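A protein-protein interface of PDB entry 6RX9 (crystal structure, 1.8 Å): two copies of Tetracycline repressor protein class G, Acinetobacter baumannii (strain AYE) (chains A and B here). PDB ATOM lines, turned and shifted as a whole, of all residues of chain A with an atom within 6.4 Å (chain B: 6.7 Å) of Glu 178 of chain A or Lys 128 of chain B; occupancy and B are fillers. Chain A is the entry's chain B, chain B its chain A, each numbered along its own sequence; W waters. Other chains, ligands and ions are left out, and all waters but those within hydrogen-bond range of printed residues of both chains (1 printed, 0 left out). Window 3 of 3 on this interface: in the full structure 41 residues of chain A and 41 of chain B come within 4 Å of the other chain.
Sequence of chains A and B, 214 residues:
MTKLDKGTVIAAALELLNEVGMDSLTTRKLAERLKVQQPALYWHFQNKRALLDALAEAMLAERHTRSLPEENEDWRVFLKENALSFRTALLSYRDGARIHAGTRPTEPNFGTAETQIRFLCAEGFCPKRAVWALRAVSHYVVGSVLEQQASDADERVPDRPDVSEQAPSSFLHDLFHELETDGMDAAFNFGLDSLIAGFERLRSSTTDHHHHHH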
ATOM      1  N   HIS A 173     -18.091  24.558 -13.839  1.00  0.00           N
ATOM      2  CA  HIS A 173     -18.729  24.029 -12.602  1.00  0.00           C
ATOM      3  C   HIS A 173     -20.172  23.599 -12.896  1.00  0.00           C
ATOM      4  O   HIS A 173     -20.551  22.483 -12.482  1.00  0.00           O
ATOM      5  CB  HIS A 173     -18.666  25.062 -11.468  1.00  0.00           C
ATOM      6  CG  HIS A 173     -19.386  24.628 -10.237  1.00  0.00           C
ATOM      7  ND1 HIS A 173     -20.631  25.122  -9.897  1.00  0.00           N
ATOM      8  CD2 HIS A 173     -19.057  23.734  -9.279  1.00  0.00           C
ATOM      9  CE1 HIS A 173     -21.031  24.562  -8.775  1.00  0.00           C
ATOM     10  NE2 HIS A 173     -20.083  23.705  -8.374  1.00  0.00           N
ATOM     11  N   ASP A 174     -20.934  24.453 -13.587  1.00  0.00           N
ATOM     12  CA  ASP A 174     -22.355  24.211 -13.961  1.00  0.00           C
ATOM     13  C   ASP A 174     -22.431  23.052 -14.964  1.00  0.00           C
ATOM     14  O   ASP A 174     -23.350  22.221 -14.827  1.00  0.00           O
ATOM     15  CB  ASP A 174     -23.000  25.479 -14.529  1.00  0.00           C
ATOM     16  CG  ASP A 174     -23.066  26.636 -13.547  1.00  0.00           C
ATOM     17  OD1 ASP A 174     -22.677  26.442 -12.376  1.00  0.00           O
ATOM     18  OD2 ASP A 174     -23.504  27.727 -13.962  1.00  0.00           O
ATOM     19  N   LEU A 175     -21.501  23.004 -15.925  1.00  0.00           N
ATOM     20  CA  LEU A 175     -21.452  21.968 -16.994  1.00  0.00           C
ATOM     21  C   LEU A 175     -21.146  20.597 -16.376  1.00  0.00           C
ATOM     22  O   LEU A 175     -21.856  19.636 -16.724  1.00  0.00           O
ATOM     23  CB  LEU A 175     -20.400  22.359 -18.041  1.00  0.00           C
ATOM     24  CG  LEU A 175     -20.239  21.396 -19.218  1.00  0.00           C
ATOM     25  CD1 LEU A 175     -21.578  21.099 -19.877  1.00  0.00           C
ATOM     26  CD2 LEU A 175     -19.257  21.950 -20.240  1.00  0.00           C
ATOM     27  N   PHE A 176     -20.140  20.514 -15.497  1.00  0.00           N
ATOM     28  CA  PHE A 176     -19.705  19.258 -14.823  1.00  0.00           C
ATOM     29  C   PHE A 176     -20.840  18.706 -13.951  1.00  0.00           C
ATOM     30  O   PHE A 176     -20.998  17.470 -13.899  1.00  0.00           O
ATOM     31  CB  PHE A 176     -18.441  19.472 -13.980  1.00  0.00           C
ATOM     32  CG  PHE A 176     -17.140  19.539 -14.745  1.00  0.00           C
ATOM     33  CD1 PHE A 176     -16.949  18.827 -15.922  1.00  0.00           C
ATOM     34  CD2 PHE A 176     -16.080  20.290 -14.257  1.00  0.00           C
ATOM     35  CE1 PHE A 176     -15.745  18.890 -16.605  1.00  0.00           C
ATOM     36  CE2 PHE A 176     -14.875  20.350 -14.941  1.00  0.00           C
ATOM     37  CZ  PHE A 176     -14.708  19.649 -16.112  1.00  0.00           C
ATOM     38  N   HIS A 177     -21.589  19.587 -13.282  1.00  0.00           N
ATOM     39  CA  HIS A 177     -22.765  19.238 -12.439  1.00  0.00           C
ATOM     40  C   HIS A 177     -23.858  18.614 -13.315  1.00  0.00           C
ATOM     41  O   HIS A 177     -24.416  17.574 -12.915  1.00  0.00           O
ATOM     42  CB  HIS A 177     -23.270  20.472 -11.680  1.00  0.00           C
ATOM     43  CG  HIS A 177     -24.479  20.208 -10.847  1.00  0.00           C
ATOM     44  ND1 HIS A 177     -25.699  20.802 -11.106  1.00  0.00           N
ATOM     45  CD2 HIS A 177     -24.666  19.407  -9.775  1.00  0.00           C
ATOM     46  CE1 HIS A 177     -26.584  20.388 -10.223  1.00  0.00           C
ATOM     47  NE2 HIS A 177     -25.975  19.529  -9.395  1.00  0.00           N
ATOM     48  N   GLU A 178     -24.137  19.234 -14.466  1.00  0.00           N
ATOM     49  CA  GLU A 178     -25.169  18.804 -15.449  1.00  0.00           C
ATOM     50  C   GLU A 178     -24.789  17.444 -16.053  1.00  0.00           C
ATOM     51  O   GLU A 178     -25.709  16.662 -16.363  1.00  0.00           O
ATOM     52  CB  GLU A 178     -25.327  19.882 -16.525  1.00  0.00           C
ATOM     53  CG  GLU A 178     -26.281  19.507 -17.641  1.00  0.00           C
ATOM     54  CD  GLU A 178     -26.745  20.679 -18.489  1.00  0.00           C
ATOM     55  OE1 GLU A 178     -25.999  21.675 -18.580  1.00  0.00           O
ATOM     56  OE2 GLU A 178     -27.854  20.595 -19.052  1.00  0.00           O
ATOM     57  N   LEU A 179     -23.488  17.177 -16.221  1.00  0.00           N
ATOM     58  CA  LEU A 179     -22.962  15.896 -16.771  1.00  0.00           C
ATOM     59  C   LEU A 179     -23.189  14.768 -15.755  1.00  0.00           C
ATOM     60  O   LEU A 179     -23.621  13.681 -16.181  1.00  0.00           O
ATOM     61  CB  LEU A 179     -21.478  16.058 -17.119  1.00  0.00           C
ATOM     62  CG  LEU A 179     -21.189  16.859 -18.388  1.00  0.00           C
ATOM     63  CD1 LEU A 179     -19.740  17.316 -18.432  1.00  0.00           C
ATOM     64  CD2 LEU A 179     -21.530  16.054 -19.632  1.00  0.00           C
ATOM     65  N   GLU A 180     -22.917  15.023 -14.470  1.00  0.00           N
ATOM     66  CA  GLU A 180     -23.145  14.061 -13.354  1.00  0.00           C
ATOM     67  C   GLU A 180     -24.631  13.687 -13.294  1.00  0.00           C
ATOM     68  O   GLU A 180     -24.929  12.493 -13.085  1.00  0.00           O
ATOM     69  CB  GLU A 180     -22.689  14.655 -12.019  1.00  0.00           C
ATOM     70  CG  GLU A 180     -21.180  14.724 -11.871  1.00  0.00           C
ATOM     71  CD  GLU A 180     -20.690  15.455 -10.633  1.00  0.00           C
ATOM     72  OE1 GLU A 180     -21.520  16.087  -9.945  1.00  0.00           O
ATOM     73  OE2 GLU A 180     -19.474  15.392 -10.357  1.00  0.00           O
ATOM     74  N   THR A 181     -25.519  14.673 -13.470  1.00  0.00           N
ATOM     75  CA  THR A 181     -27.000  14.515 -13.468  1.00  0.00           C
ATOM     76  C   THR A 181     -27.418  13.534 -14.573  1.00  0.00           C
ATOM     77  O   THR A 181     -28.252  12.653 -14.286  1.00  0.00           O
ATOM     78  CB  THR A 181     -27.697  15.875 -13.617  1.00  0.00           C
ATOM     79  OG1 THR A 181     -27.185  16.749 -12.610  1.00  0.00           O
ATOM     80  CG2 THR A 181     -29.203  15.791 -13.495  1.00  0.00           C
ATOM     81  N   ASP A 182     -26.855  13.679 -15.779  1.00  0.00           N
ATOM     82  CA  ASP A 182     -27.174  12.845 -16.972  1.00  0.00           C
ATOM     83  C   ASP A 182     -26.811  11.377 -16.708  1.00  0.00           C
ATOM     84  O   ASP A 182     -27.552  10.499 -17.191  1.00  0.00           O
ATOM     85  CB  ASP A 182     -26.470  13.359 -18.232  1.00  0.00           C
ATOM     86  CG  ASP A 182     -27.323  14.306 -19.056  1.00  0.00           C
ATOM     87  OD1 ASP A 182     -27.812  15.297 -18.485  1.00  0.00           O
ATOM     88  OD2 ASP A 182     -27.504  14.033 -20.259  1.00  0.00           O
ATOM     89  N   GLY A 183     -25.707  11.127 -15.995  1.00  0.00           N
ATOM     90  CA  GLY A 183     -25.277   9.778 -15.572  1.00  0.00           C
ATOM     91  C   GLY A 183     -24.203   9.203 -16.483  1.00  0.00           C
ATOM     92  O   GLY A 183     -23.973   9.771 -17.572  1.00  0.00           O
ATOM     93  N   ILE B 117     -13.579  22.827 -25.048  1.00  0.00           N
ATOM     94  CA  ILE B 117     -15.070  22.714 -25.001  1.00  0.00           C
ATOM     95  C   ILE B 117     -15.692  23.891 -25.767  1.00  0.00           C
ATOM     96  O   ILE B 117     -16.578  23.642 -26.607  1.00  0.00           O
ATOM     97  CB  ILE B 117     -15.575  22.631 -23.544  1.00  0.00           C
ATOM     98  CG1 ILE B 117     -15.121  21.337 -22.862  1.00  0.00           C
ATOM     99  CG2 ILE B 117     -17.089  22.794 -23.482  1.00  0.00           C
ATOM    100  CD1 ILE B 117     -15.199  21.371 -21.353  1.00  0.00           C
ATOM    101  N   CYS B 121     -18.047  23.848 -29.176  1.00  0.00           N
ATOM    102  CA  CYS B 121     -19.357  24.552 -29.108  1.00  0.00           C
ATOM    103  C   CYS B 121     -19.486  25.520 -30.291  1.00  0.00           C
ATOM    104  O   CYS B 121     -20.564  25.539 -30.920  1.00  0.00           O
ATOM    105  CB  CYS B 121     -19.540  25.281 -27.782  1.00  0.00           C
ATOM    106  SG  CYS B 121     -19.853  24.153 -26.398  1.00  0.00           S
ATOM    107  N   PHE B 125     -21.125  21.729 -31.684  1.00  0.00           N
ATOM    108  CA  PHE B 125     -21.385  20.785 -30.562  1.00  0.00           C
ATOM    109  C   PHE B 125     -22.184  21.511 -29.474  1.00  0.00           C
ATOM    110  O   PHE B 125     -21.979  22.725 -29.296  1.00  0.00           O
ATOM    111  CB  PHE B 125     -20.086  20.251 -29.951  1.00  0.00           C
ATOM    112  CG  PHE B 125     -19.371  19.197 -30.756  1.00  0.00           C
ATOM    113  CD1 PHE B 125     -18.611  19.540 -31.864  1.00  0.00           C
ATOM    114  CD2 PHE B 125     -19.436  17.860 -30.391  1.00  0.00           C
ATOM    115  CE1 PHE B 125     -17.946  18.568 -32.597  1.00  0.00           C
ATOM    116  CE2 PHE B 125     -18.769  16.890 -31.123  1.00  0.00           C
ATOM    117  CZ  PHE B 125     -18.023  17.246 -32.223  1.00  0.00           C
ATOM    118  N   CYS B 126     -23.062  20.793 -28.768  1.00  0.00           N
ATOM    119  CA  CYS B 126     -23.668  21.258 -27.491  1.00  0.00           C
ATOM    120  C   CYS B 126     -22.668  20.973 -26.371  1.00  0.00           C
ATOM    121  O   CYS B 126     -21.918  20.003 -26.455  1.00  0.00           O
ATOM    122  CB  CYS B 126     -25.021  20.603 -27.236  1.00  0.00           C
ATOM    123  SG  CYS B 126     -24.963  19.220 -26.068  1.00  0.00           S
ATOM    124  N   PRO B 127     -22.599  21.815 -25.310  1.00  0.00           N
ATOM    125  CA  PRO B 127     -21.580  21.674 -24.266  1.00  0.00           C
ATOM    126  C   PRO B 127     -21.389  20.252 -23.710  1.00  0.00           C
ATOM    127  O   PRO B 127     -20.251  19.835 -23.566  1.00  0.00           O
ATOM    128  CB  PRO B 127     -22.103  22.597 -23.156  1.00  0.00           C
ATOM    129  CG  PRO B 127     -22.841  23.682 -23.906  1.00  0.00           C
ATOM    130  CD  PRO B 127     -23.491  22.964 -25.070  1.00  0.00           C
ATOM    131  N   LYS B 128     -22.492  19.564 -23.394  1.00  0.00           N
ATOM    132  CA  LYS B 128     -22.498  18.162 -22.889  1.00  0.00           C
ATOM    133  C   LYS B 128     -21.751  17.259 -23.874  1.00  0.00           C
ATOM    134  O   LYS B 128     -20.825  16.545 -23.445  1.00  0.00           O
ATOM    135  CB  LYS B 128     -23.921  17.614 -22.756  1.00  0.00           C
ATOM    136  CG  LYS B 128     -24.632  17.895 -21.442  1.00  0.00           C
ATOM    137  CD  LYS B 128     -25.879  17.044 -21.289  1.00  0.00           C
ATOM    138  CE  LYS B 128     -26.959  17.687 -20.448  1.00  0.00           C
ATOM    139  NZ  LYS B 128     -28.309  17.235 -20.859  1.00  0.00           N
ATOM    140  N   ARG B 129     -22.174  17.287 -25.140  1.00  0.00           N
ATOM    141  CA  ARG B 129     -21.725  16.348 -26.201  1.00  0.00           C
ATOM    142  C   ARG B 129     -20.273  16.658 -26.575  1.00  0.00           C
ATOM    143  O   ARG B 129     -19.561  15.713 -26.954  1.00  0.00           O
ATOM    144  CB  ARG B 129     -22.696  16.396 -27.385  1.00  0.00           C
ATOM    145  CG  ARG B 129     -24.038  15.749 -27.072  1.00  0.00           C
ATOM    146  CD  ARG B 129     -25.119  16.025 -28.096  1.00  0.00           C
ATOM    147  NE  ARG B 129     -26.393  15.439 -27.688  1.00  0.00           N
ATOM    148  CZ  ARG B 129     -27.013  14.418 -28.283  1.00  0.00           C
ATOM    149  NH1 ARG B 129     -26.500  13.835 -29.355  1.00  0.00           N
ATOM    150  NH2 ARG B 129     -28.168  13.989 -27.803  1.00  0.00           N
ATOM    151  N   ALA B 130     -19.843  17.918 -26.436  1.00  0.00           N
ATOM    152  CA  ALA B 130     -18.427  18.336 -26.577  1.00  0.00           C
ATOM    153  C   ALA B 130     -17.564  17.558 -25.574  1.00  0.00           C
ATOM    154  O   ALA B 130     -16.546  16.983 -25.994  1.00  0.00           O
ATOM    155  CB  ALA B 130     -18.293  19.828 -26.387  1.00  0.00           C
ATOM    156  N   VAL B 131     -17.968  17.525 -24.299  1.00  0.00           N
ATOM    157  CA  VAL B 131     -17.229  16.813 -23.213  1.00  0.00           C
ATOM    158  C   VAL B 131     -17.279  15.302 -23.488  1.00  0.00           C
ATOM    159  O   VAL B 131     -16.228  14.651 -23.350  1.00  0.00           O
ATOM    160  CB  VAL B 131     -17.773  17.154 -21.813  1.00  0.00           C
ATOM    161  CG1 VAL B 131     -17.129  16.293 -20.735  1.00  0.00           C
ATOM    162  CG2 VAL B 131     -17.599  18.632 -21.484  1.00  0.00           C
ATOM    163  N   TRP B 132     -18.449  14.772 -23.862  1.00  0.00           N
ATOM    164  CA  TRP B 132     -18.644  13.326 -24.169  1.00  0.00           C
ATOM    165  C   TRP B 132     -17.730  12.903 -25.325  1.00  0.00           C
ATOM    166  O   TRP B 132     -17.182  11.790 -25.258  1.00  0.00           O
ATOM    167  CB  TRP B 132     -20.110  13.009 -24.482  1.00  0.00           C
ATOM    168  CG  TRP B 132     -21.031  13.073 -23.304  1.00  0.00           C
ATOM    169  CD1 TRP B 132     -20.690  13.089 -21.982  1.00  0.00           C
ATOM    170  CD2 TRP B 132     -22.468  13.085 -23.345  1.00  0.00           C
ATOM    171  NE1 TRP B 132     -21.813  13.135 -21.202  1.00  0.00           N
ATOM    172  CE2 TRP B 132     -22.918  13.128 -22.009  1.00  0.00           C
ATOM    173  CE3 TRP B 132     -23.414  13.072 -24.377  1.00  0.00           C
ATOM    174  CZ2 TRP B 132     -24.273  13.162 -21.682  1.00  0.00           C
ATOM    175  CZ3 TRP B 132     -24.753  13.101 -24.054  1.00  0.00           C
ATOM    176  CH2 TRP B 132     -25.173  13.145 -22.723  1.00  0.00           C
ATOM    177  N   ALA B 133     -17.590  13.756 -26.347  1.00  0.00           N
ATOM    178  CA  ALA B 133     -16.768  13.514 -27.556  1.00  0.00           C
ATOM    179  C   ALA B 133     -15.282  13.485 -27.183  1.00  0.00           C
ATOM    180  O   ALA B 133     -14.593  12.526 -27.574  1.00  0.00           O
ATOM    181  CB  ALA B 133     -17.055  14.569 -28.599  1.00  0.00           C
HETATM  182  O   HOH W   1     -23.004  12.193 -18.405  1.00  0.00           O
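The side-chain carboxylate (OE2) of Glu 178 of chain A is in salt-bridge range of the side-chain amino group (NZ) of Lys 128 of chain B (3.8 Å). OD1 of Asp 182 of chain A is in salt-bridge range of NZ of Lys 128 of chain B (3.1 Å).
The backbone carbonyl oxygen (O) of Ile 117 of chain B sits at hydrogen-bond distance from the side-chain sulfur (SG) of Cys 121 of chain B (3.3 Å). The side-chain sulfur of Cys 126 of chain B lies close to the backbone NH of Lys 128 of chain B, 3.7 Å away.
Leu 175 of chain A touches Ile 117 of chain B. Leu 175 of chain A touches Pro 127 of chain B (CD1 to CB, 3.6 Å). Leu 175 of chain A touches Lys 128 of chain B. CG2 of Val 131 of chain B touches CD2 of Leu 175 of chain A, at 3.9 Å. Leu 179 of chain A touches Lys 128 of chain B. Leu 179 of chain A touches Val 131 of chain B (CD1 to CG1, 3.6 Å). Leu 179 of chain A touches Trp 132 of chain B. Trp 132 of chain B touches Asp 182 of chain A.
Of the printed residues of chain B, Glu 178 of chain A touches Lys 128. Glu 180 of chain A touches none of the printed residues of chain B. Printed residues of chain B within 4 Å of Asp 182 of chain A: Lys 128 and Trp 132. Of the printed residues of chain A, Ile 117 of chain B touches Leu 175 (3.99 Å). Of the printed residues of chain A, Pro 127 of chain B touches Leu 175. Of the printed residues of chain A, Lys 128 of chain B touches Leu 175 (3.9 Å), Glu 178 (3.3 Å), Leu 179 (3.9 Å) and Asp 182 (3.1 Å). Ala 130 of chain B touches none of the printed residues of chain A. Printed residues of chain A within 4 Å of Val 131 of chain B: Leu 175 and Leu 179. Of the printed residues of chain A, Trp 132 of chain B touches Leu 179 and Asp 182. The nearest printed residue of chain A that does not touch Lys 128 of chain B is Thr 181 of chain A (7.1 Å). The nearest printed residue of chain B that does not touch Leu 175 of chain A is Arg 129 of chain B (6.5 Å).
Of the 11 printed residues of chain A, 4 touch a printed residue of chain B. Hydrophobic or aromatic side chains of chain A within 4 Å of the printed part of chain B: Leu 175 and Leu 179. Along chain A the printed residues that touch a printed residue of chain B span positions 175 to 182. Among the printed residues, 10 pairs touch across the chains.
No position is printed for both chains.
Water W1 lies within hydrogen-bond range of the backbone carbonyl oxygen (O) of Gly 183 of chain A (2.7 Å), the backbone carbonyl oxygen (O) of Leu 179 of chain A (2.7 Å) and the indole nitrogen (NE1) of Trp 132 of chain B (3.2 Å).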
